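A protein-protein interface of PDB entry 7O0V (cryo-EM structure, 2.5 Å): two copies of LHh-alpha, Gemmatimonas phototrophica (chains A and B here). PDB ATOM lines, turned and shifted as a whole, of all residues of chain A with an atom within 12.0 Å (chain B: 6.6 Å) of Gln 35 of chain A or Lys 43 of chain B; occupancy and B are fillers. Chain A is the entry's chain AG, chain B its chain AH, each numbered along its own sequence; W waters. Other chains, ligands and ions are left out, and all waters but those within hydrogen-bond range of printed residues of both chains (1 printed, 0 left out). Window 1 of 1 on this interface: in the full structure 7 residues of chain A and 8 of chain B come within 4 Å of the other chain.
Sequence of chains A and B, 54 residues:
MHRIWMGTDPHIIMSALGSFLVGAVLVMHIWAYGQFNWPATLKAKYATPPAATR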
ATOM      1  N   LEU A  26      21.127  24.318  -0.421  1.00  0.00           N
ATOM      2  CA  LEU A  26      20.694  24.182   0.968  1.00  0.00           C
ATOM      3  C   LEU A  26      20.274  25.525   1.556  1.00  0.00           C
ATOM      4  O   LEU A  26      19.233  25.625   2.216  1.00  0.00           O
ATOM      5  CB  LEU A  26      21.804  23.553   1.809  1.00  0.00           C
ATOM      6  CG  LEU A  26      22.100  22.072   1.574  1.00  0.00           C
ATOM      7  CD1 LEU A  26      23.301  21.638   2.390  1.00  0.00           C
ATOM      8  CD2 LEU A  26      20.888  21.221   1.911  1.00  0.00           C
ATOM      9  N   VAL A  27      21.075  26.566   1.334  1.00  0.00           N
ATOM     10  CA  VAL A  27      20.723  27.905   1.807  1.00  0.00           C
ATOM     11  C   VAL A  27      19.386  28.355   1.227  1.00  0.00           C
ATOM     12  O   VAL A  27      18.514  28.858   1.947  1.00  0.00           O
ATOM     13  CB  VAL A  27      21.847  28.903   1.478  1.00  0.00           C
ATOM     14  CG1 VAL A  27      21.337  30.332   1.558  1.00  0.00           C
ATOM     15  CG2 VAL A  27      23.014  28.707   2.430  1.00  0.00           C
ATOM     16  N   MET A  28      19.204  28.182  -0.084  1.00  0.00           N
ATOM     17  CA  MET A  28      17.951  28.571  -0.726  1.00  0.00           C
ATOM     18  C   MET A  28      16.744  27.814  -0.180  1.00  0.00           C
ATOM     19  O   MET A  28      15.677  28.405   0.015  1.00  0.00           O
ATOM     20  CB  MET A  28      18.059  28.375  -2.237  1.00  0.00           C
ATOM     21  CG  MET A  28      18.875  29.445  -2.948  1.00  0.00           C
ATOM     22  SD  MET A  28      18.388  31.132  -2.529  1.00  0.00           S
ATOM     23  CE  MET A  28      16.645  31.107  -2.935  1.00  0.00           C
ATOM     24  N   HIS A  29      16.882  26.511   0.079  1.00  0.00           N
ATOM     25  CA  HIS A  29      15.755  25.764   0.635  1.00  0.00           C
ATOM     26  C   HIS A  29      15.452  26.150   2.078  1.00  0.00           C
ATOM     27  O   HIS A  29      14.278  26.272   2.448  1.00  0.00           O
ATOM     28  CB  HIS A  29      15.977  24.258   0.495  1.00  0.00           C
ATOM     29  CG  HIS A  29      15.746  23.750  -0.895  1.00  0.00           C
ATOM     30  ND1 HIS A  29      16.613  23.993  -1.938  1.00  0.00           N
ATOM     31  CD2 HIS A  29      14.716  23.046  -1.420  1.00  0.00           C
ATOM     32  CE1 HIS A  29      16.137  23.440  -3.040  1.00  0.00           C
ATOM     33  NE2 HIS A  29      14.986  22.860  -2.754  1.00  0.00           N
ATOM     34  N   ILE A  30      16.475  26.335   2.914  1.00  0.00           N
ATOM     35  CA  ILE A  30      16.212  26.766   4.287  1.00  0.00           C
ATOM     36  C   ILE A  30      15.498  28.109   4.280  1.00  0.00           C
ATOM     37  O   ILE A  30      14.525  28.321   5.013  1.00  0.00           O
ATOM     38  CB  ILE A  30      17.518  26.839   5.098  1.00  0.00           C
ATOM     39  CG1 ILE A  30      18.172  25.467   5.209  1.00  0.00           C
ATOM     40  CG2 ILE A  30      17.252  27.399   6.485  1.00  0.00           C
ATOM     41  CD1 ILE A  30      19.620  25.536   5.637  1.00  0.00           C
ATOM     42  N   TRP A  31      15.970  29.031   3.442  1.00  0.00           N
ATOM     43  CA  TRP A  31      15.334  30.334   3.303  1.00  0.00           C
ATOM     44  C   TRP A  31      13.902  30.194   2.795  1.00  0.00           C
ATOM     45  O   TRP A  31      12.965  30.748   3.382  1.00  0.00           O
ATOM     46  CB  TRP A  31      16.179  31.207   2.373  1.00  0.00           C
ATOM     47  CG  TRP A  31      15.639  32.574   2.120  1.00  0.00           C
ATOM     48  CD1 TRP A  31      15.899  33.700   2.842  1.00  0.00           C
ATOM     49  CD2 TRP A  31      14.783  32.976   1.045  1.00  0.00           C
ATOM     50  NE1 TRP A  31      15.242  34.774   2.298  1.00  0.00           N
ATOM     51  CE2 TRP A  31      14.550  34.357   1.192  1.00  0.00           C
ATOM     52  CE3 TRP A  31      14.183  32.301  -0.021  1.00  0.00           C
ATOM     53  CZ2 TRP A  31      13.744  35.075   0.313  1.00  0.00           C
ATOM     54  CZ3 TRP A  31      13.383  33.015  -0.892  1.00  0.00           C
ATOM     55  CH2 TRP A  31      13.170  34.387  -0.719  1.00  0.00           C
ATOM     56  N   ALA A  32      13.714  29.451   1.701  1.00  0.00           N
ATOM     57  CA  ALA A  32      12.392  29.320   1.091  1.00  0.00           C
ATOM     58  C   ALA A  32      11.400  28.602   2.004  1.00  0.00           C
ATOM     59  O   ALA A  32      10.221  28.970   2.043  1.00  0.00           O
ATOM     60  CB  ALA A  32      12.501  28.596  -0.249  1.00  0.00           C
ATOM     61  N   TYR A  33      11.846  27.576   2.739  1.00  0.00           N
ATOM     62  CA  TYR A  33      10.951  26.920   3.691  1.00  0.00           C
ATOM     63  C   TYR A  33      10.408  27.895   4.726  1.00  0.00           C
ATOM     64  O   TYR A  33       9.291  27.716   5.221  1.00  0.00           O
ATOM     65  CB  TYR A  33      11.660  25.775   4.420  1.00  0.00           C
ATOM     66  CG  TYR A  33      12.047  24.570   3.592  1.00  0.00           C
ATOM     67  CD1 TYR A  33      11.536  24.369   2.318  1.00  0.00           C
ATOM     68  CD2 TYR A  33      12.911  23.614   4.110  1.00  0.00           C
ATOM     69  CE1 TYR A  33      11.898  23.257   1.575  1.00  0.00           C
ATOM     70  CE2 TYR A  33      13.270  22.504   3.381  1.00  0.00           C
ATOM     71  CZ  TYR A  33      12.765  22.329   2.114  1.00  0.00           C
ATOM     72  OH  TYR A  33      13.123  21.217   1.390  1.00  0.00           O
ATOM     73  N   GLY A  34      11.176  28.926   5.060  1.00  0.00           N
ATOM     74  CA  GLY A  34      10.723  29.971   5.954  1.00  0.00           C
ATOM     75  C   GLY A  34       9.671  30.876   5.354  1.00  0.00           C
ATOM     76  O   GLY A  34       8.585  31.035   5.918  1.00  0.00           O
ATOM     77  N   GLN A  35       9.987  31.478   4.207  1.00  0.00           N
ATOM     78  CA  GLN A  35       9.086  32.450   3.598  1.00  0.00           C
ATOM     79  C   GLN A  35       7.766  31.812   3.179  1.00  0.00           C
ATOM     80  O   GLN A  35       6.690  32.366   3.426  1.00  0.00           O
ATOM     81  CB  GLN A  35       9.763  33.103   2.391  1.00  0.00           C
ATOM     82  CG  GLN A  35      11.206  33.568   2.596  1.00  0.00           C
ATOM     83  CD  GLN A  35      11.441  34.302   3.906  1.00  0.00           C
ATOM     84  OE1 GLN A  35      10.580  35.030   4.394  1.00  0.00           O
ATOM     85  NE2 GLN A  35      12.625  34.117   4.474  1.00  0.00           N
ATOM     86  N   PHE A  36       7.826  30.644   2.542  1.00  0.00           N
ATOM     87  CA  PHE A  36       6.643  30.057   1.923  1.00  0.00           C
ATOM     88  C   PHE A  36       5.777  29.241   2.876  1.00  0.00           C
ATOM     89  O   PHE A  36       4.749  28.713   2.440  1.00  0.00           O
ATOM     90  CB  PHE A  36       7.061  29.223   0.713  1.00  0.00           C
ATOM     91  CG  PHE A  36       7.473  30.061  -0.460  1.00  0.00           C
ATOM     92  CD1 PHE A  36       8.752  30.581  -0.540  1.00  0.00           C
ATOM     93  CD2 PHE A  36       6.568  30.365  -1.460  1.00  0.00           C
ATOM     94  CE1 PHE A  36       9.125  31.370  -1.608  1.00  0.00           C
ATOM     95  CE2 PHE A  36       6.935  31.151  -2.530  1.00  0.00           C
ATOM     96  CZ  PHE A  36       8.216  31.656  -2.603  1.00  0.00           C
ATOM     97  N   ASN A  37       6.163  29.119   4.148  1.00  0.00           N
ATOM     98  CA  ASN A  37       5.399  28.368   5.149  1.00  0.00           C
ATOM     99  C   ASN A  37       5.183  26.905   4.756  1.00  0.00           C
ATOM    100  O   ASN A  37       4.179  26.294   5.127  1.00  0.00           O
ATOM    101  CB  ASN A  37       4.057  29.055   5.429  1.00  0.00           C
ATOM    102  CG  ASN A  37       3.487  28.703   6.785  1.00  0.00           C
ATOM    103  OD1 ASN A  37       4.223  28.401   7.721  1.00  0.00           O
ATOM    104  ND2 ASN A  37       2.166  28.752   6.901  1.00  0.00           N
ATOM    105  N   TRP A  38       6.118  26.331   4.004  1.00  0.00           N
ATOM    106  CA  TRP A  38       6.087  24.920   3.645  1.00  0.00           C
ATOM    107  C   TRP A  38       7.451  24.329   3.981  1.00  0.00           C
ATOM    108  O   TRP A  38       8.481  24.945   3.661  1.00  0.00           O
ATOM    109  CB  TRP A  38       5.773  24.731   2.156  1.00  0.00           C
ATOM    110  CG  TRP A  38       5.492  23.312   1.754  1.00  0.00           C
ATOM    111  CD1 TRP A  38       4.266  22.747   1.575  1.00  0.00           C
ATOM    112  CD2 TRP A  38       6.451  22.282   1.475  1.00  0.00           C
ATOM    113  NE1 TRP A  38       4.396  21.433   1.206  1.00  0.00           N
ATOM    114  CE2 TRP A  38       5.728  21.122   1.139  1.00  0.00           C
ATOM    115  CE3 TRP A  38       7.848  22.228   1.482  1.00  0.00           C
ATOM    116  CZ2 TRP A  38       6.352  19.924   0.810  1.00  0.00           C
ATOM    117  CZ3 TRP A  38       8.465  21.035   1.159  1.00  0.00           C
ATOM    118  CH2 TRP A  38       7.717  19.900   0.827  1.00  0.00           C
ATOM    119  N   PRO A  39       7.521  23.146   4.613  1.00  0.00           N
ATOM    120  CA  PRO A  39       6.511  22.120   4.895  1.00  0.00           C
ATOM    121  C   PRO A  39       5.612  22.342   6.116  1.00  0.00           C
ATOM    122  O   PRO A  39       4.913  21.405   6.491  1.00  0.00           O
ATOM    123  CB  PRO A  39       7.370  20.871   5.110  1.00  0.00           C
ATOM    124  CG  PRO A  39       8.561  21.412   5.796  1.00  0.00           C
ATOM    125  CD  PRO A  39       8.856  22.685   5.031  1.00  0.00           C
ATOM    126  N   ALA A  40       5.641  23.525   6.733  1.00  0.00           N
ATOM    127  CA  ALA A  40       4.810  23.757   7.913  1.00  0.00           C
ATOM    128  C   ALA A  40       3.326  23.503   7.650  1.00  0.00           C
ATOM    129  O   ALA A  40       2.638  22.918   8.493  1.00  0.00           O
ATOM    130  CB  ALA A  40       5.022  25.181   8.426  1.00  0.00           C
ATOM    131  N   THR A  41       2.811  23.925   6.491  1.00  0.00           N
ATOM    132  CA  THR A  41       1.431  23.583   6.144  1.00  0.00           C
ATOM    133  C   THR A  41       1.245  22.098   5.851  1.00  0.00           C
ATOM    134  O   THR A  41       0.174  21.548   6.127  1.00  0.00           O
ATOM    135  CB  THR A  41       0.949  24.414   4.952  1.00  0.00           C
ATOM    136  OG1 THR A  41       1.791  24.179   3.819  1.00  0.00           O
ATOM    137  CG2 THR A  41       0.943  25.893   5.296  1.00  0.00           C
ATOM    138  N   LEU A  42       2.261  21.435   5.296  1.00  0.00           N
ATOM    139  CA  LEU A  42       2.206  19.983   5.142  1.00  0.00           C
ATOM    140  C   LEU A  42       2.110  19.280   6.492  1.00  0.00           C
ATOM    141  O   LEU A  42       1.295  18.369   6.674  1.00  0.00           O
ATOM    142  CB  LEU A  42       3.424  19.497   4.355  1.00  0.00           C
ATOM    143  CG  LEU A  42       3.823  18.028   4.498  1.00  0.00           C
ATOM    144  CD1 LEU A  42       2.755  17.125   3.912  1.00  0.00           C
ATOM    145  CD2 LEU A  42       5.159  17.772   3.824  1.00  0.00           C
ATOM    146  N   PRO B  39      11.576  39.773   1.489  1.00  0.00           N
ATOM    147  CA  PRO B  39      10.426  38.860   1.464  1.00  0.00           C
ATOM    148  C   PRO B  39       9.388  39.012   2.580  1.00  0.00           C
ATOM    149  O   PRO B  39       8.473  38.196   2.636  1.00  0.00           O
ATOM    150  CB  PRO B  39      11.094  37.486   1.565  1.00  0.00           C
ATOM    151  CG  PRO B  39      12.264  37.746   2.432  1.00  0.00           C
ATOM    152  CD  PRO B  39      12.794  39.062   1.914  1.00  0.00           C
ATOM    153  N   ALA B  40       9.539  40.004   3.459  1.00  0.00           N
ATOM    154  CA  ALA B  40       8.638  40.138   4.603  1.00  0.00           C
ATOM    155  C   ALA B  40       7.156  40.170   4.221  1.00  0.00           C
ATOM    156  O   ALA B  40       6.320  39.615   4.943  1.00  0.00           O
ATOM    157  CB  ALA B  40       8.998  41.394   5.396  1.00  0.00           C
ATOM    158  N   THR B  41       6.802  40.808   3.102  1.00  0.00           N
ATOM    159  CA  THR B  41       5.418  40.721   2.629  1.00  0.00           C
ATOM    160  C   THR B  41       5.072  39.347   2.064  1.00  0.00           C
ATOM    161  O   THR B  41       3.942  38.874   2.227  1.00  0.00           O
ATOM    162  CB  THR B  41       5.130  41.808   1.590  1.00  0.00           C
ATOM    163  OG1 THR B  41       6.047  41.697   0.496  1.00  0.00           O
ATOM    164  CG2 THR B  41       5.231  43.188   2.213  1.00  0.00           C
ATOM    165  N   LEU B  42       6.021  38.692   1.392  1.00  0.00           N
ATOM    166  CA  LEU B  42       5.812  37.308   0.969  1.00  0.00           C
ATOM    167  C   LEU B  42       5.546  36.386   2.154  1.00  0.00           C
ATOM    168  O   LEU B  42       4.626  35.561   2.118  1.00  0.00           O
ATOM    169  CB  LEU B  42       7.015  36.825   0.157  1.00  0.00           C
ATOM    170  CG  LEU B  42       7.274  35.319   0.079  1.00  0.00           C
ATOM    171  CD1 LEU B  42       6.167  34.618  -0.688  1.00  0.00           C
ATOM    172  CD2 LEU B  42       8.621  35.050  -0.566  1.00  0.00           C
ATOM    173  N   LYS B  43       6.348  36.505   3.214  1.00  0.00           N
ATOM    174  CA  LYS B  43       6.150  35.670   4.396  1.00  0.00           C
ATOM    175  C   LYS B  43       4.771  35.880   5.017  1.00  0.00           C
ATOM    176  O   LYS B  43       4.087  34.915   5.373  1.00  0.00           O
ATOM    177  CB  LYS B  43       7.248  35.945   5.422  1.00  0.00           C
ATOM    178  CG  LYS B  43       7.286  34.925   6.543  1.00  0.00           C
ATOM    179  CD  LYS B  43       8.396  35.206   7.533  1.00  0.00           C
ATOM    180  CE  LYS B  43       8.462  34.112   8.584  1.00  0.00           C
ATOM    181  NZ  LYS B  43       9.446  34.419   9.657  1.00  0.00           N
ATOM    182  N   ALA B  44       4.352  37.138   5.161  1.00  0.00           N
ATOM    183  CA  ALA B  44       3.031  37.437   5.709  1.00  0.00           C
ATOM    184  C   ALA B  44       1.906  36.845   4.865  1.00  0.00           C
ATOM    185  O   ALA B  44       0.917  36.339   5.406  1.00  0.00           O
ATOM    186  CB  ALA B  44       2.856  38.950   5.843  1.00  0.00           C
ATOM    187  N   LYS B  45       2.038  36.908   3.540  1.00  0.00           N
ATOM    188  CA  LYS B  45       1.024  36.368   2.636  1.00  0.00           C
ATOM    189  C   LYS B  45       0.694  34.899   2.899  1.00  0.00           C
ATOM    190  O   LYS B  45      -0.462  34.494   2.739  1.00  0.00           O
ATOM    191  CB  LYS B  45       1.500  36.545   1.193  1.00  0.00           C
ATOM    192  CG  LYS B  45       0.486  36.198   0.122  1.00  0.00           C
ATOM    193  CD  LYS B  45       1.037  36.541  -1.255  1.00  0.00           C
ATOM    194  CE  LYS B  45       0.077  36.147  -2.365  1.00  0.00           C
ATOM    195  NZ  LYS B  45      -1.168  36.962  -2.349  1.00  0.00           N
ATOM    196  N   TYR B  46       1.673  34.089   3.298  1.00  0.00           N
ATOM    197  CA  TYR B  46       1.444  32.670   3.546  1.00  0.00           C
ATOM    198  C   TYR B  46       1.494  32.261   5.014  1.00  0.00           C
ATOM    199  O   TYR B  46       1.308  31.076   5.314  1.00  0.00           O
ATOM    200  CB  TYR B  46       2.428  31.845   2.710  1.00  0.00           C
ATOM    201  CG  TYR B  46       2.206  32.097   1.238  1.00  0.00           C
ATOM    202  CD1 TYR B  46       1.012  31.732   0.632  1.00  0.00           C
ATOM    203  CD2 TYR B  46       3.157  32.750   0.467  1.00  0.00           C
ATOM    204  CE1 TYR B  46       0.786  31.971  -0.705  1.00  0.00           C
ATOM    205  CE2 TYR B  46       2.935  33.001  -0.874  1.00  0.00           C
ATOM    206  CZ  TYR B  46       1.748  32.607  -1.454  1.00  0.00           C
ATOM    207  OH  TYR B  46       1.512  32.859  -2.784  1.00  0.00           O
ATOM    208  N   ALA B  47       1.748  33.191   5.931  1.00  0.00           N
ATOM    209  CA  ALA B  47       1.842  32.848   7.346  1.00  0.00           C
ATOM    210  C   ALA B  47       0.516  32.320   7.887  1.00  0.00           C
ATOM    211  O   ALA B  47      -0.564  32.765   7.486  1.00  0.00           O
ATOM    212  CB  ALA B  47       2.284  34.068   8.153  1.00  0.00           C
ATOM    213  N   THR B  48       0.609  31.360   8.803  1.00  0.00           N
ATOM    214  CA  THR B  48      -0.568  30.752   9.420  1.00  0.00           C
ATOM    215  C   THR B  48      -1.132  31.660  10.506  1.00  0.00           C
ATOM    216  O   THR B  48      -0.431  31.948  11.482  1.00  0.00           O
ATOM    217  CB  THR B  48      -0.215  29.397  10.019  1.00  0.00           C
ATOM    218  OG1 THR B  48       0.287  28.533   8.992  1.00  0.00           O
ATOM    219  CG2 THR B  48      -1.438  28.759  10.662  1.00  0.00           C
HETATM  220  O   HOH W   1       5.068  32.374   5.626  1.00  0.00           O
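Positions printed for both chains: 39, 40, 41 and 42.
Among the printed residues, pairs that only touch across the chains: Trp 31 of chain A with Pro 39 of chain B (3.7 Å), Gln 35 of chain A with Pro 39 of chain B (3.7 Å), Gln 35 of chain A with Leu 42 of chain B (3.7 Å), Gln 35 of chain A with Lys 43 of chain B (3.5 Å), Phe 36 of chain A with Leu 42 of chain B (3.9 Å) and Phe 36 of chain A with Tyr 46 of chain B (3.9 Å).
The backbone carbonyl oxygen (O) of Tyr 46 of chain B sits at hydrogen-bond distance from the side-chain amide nitrogen (ND2) of Asn 37 of chain A (2.9 Å).
The side-chain hydroxyl of Thr 48 of chain B is in hydrogen-bond range of the side-chain amide nitrogen of Asn 37 of chain A (2.8 Å).
Gln 35 of chain A touches just these residues of chain B: Pro 39, Leu 42 and Lys 43.
Of the printed residues of chain A, Lys 43 of chain B touches Gln 35.
No residue of chain A comes within 4 Å of Ala 40 of chain B.
No residue of chain A comes within 4 Å of Thr 41 of chain B.
No residue of chain A comes within 4 Å of Ala 44 of chain B.
Of the printed residues of chain B, Asn 37 of chain A touches Tyr 46 (2.9 Å) and Thr 48 (2.8 Å).
Printed residues of chain A within 4 Å of Thr 48 of chain B: Asn 37.
Of the printed residues of chain B, Trp 31 of chain A touches Pro 39.
The nearest residue of chain A that does not touch Lys 43 of chain B is Gly 34 of chain A (4.1 Å).
The nearest printed residue of chain A that does not touch Tyr 46 of chain B is Gln 35 of chain A (4.4 Å).
Of the 10 printed residues of chain B, 5 touch a printed residue of chain A.
Of the 17 printed residues of chain A, 4 touch a printed residue of chain B.
Printed residues of chain A that touch a printed residue of chain B: Trp 31, Gln 35, Phe 36 and Asn 37.
Hydrophobic or aromatic side chains of chain A that line the printed part of chain B: Trp 31 and Phe 36.
Among the printed residues, no Asp or Glu carboxylate lies within 4 Å of a Lys or Arg side-chain nitrogen of the other chain.
NE1 of Trp 31 of chain A lies close to NE2 of Gln 35 of chain A (3.5 Å).
O of Asn 37 of chain A sits close to OG1 of Thr 41 of chain A (3.4 Å).
Water W1 lies within hydrogen-bond range of the backbone carbonyl oxygen of Gln 35 of chain A (2.7 Å), the backbone carbonyl oxygen of Lys 43 of chain B (2.7 Å) and the backbone NH of Ala 47 of chain B (3.4 Å).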
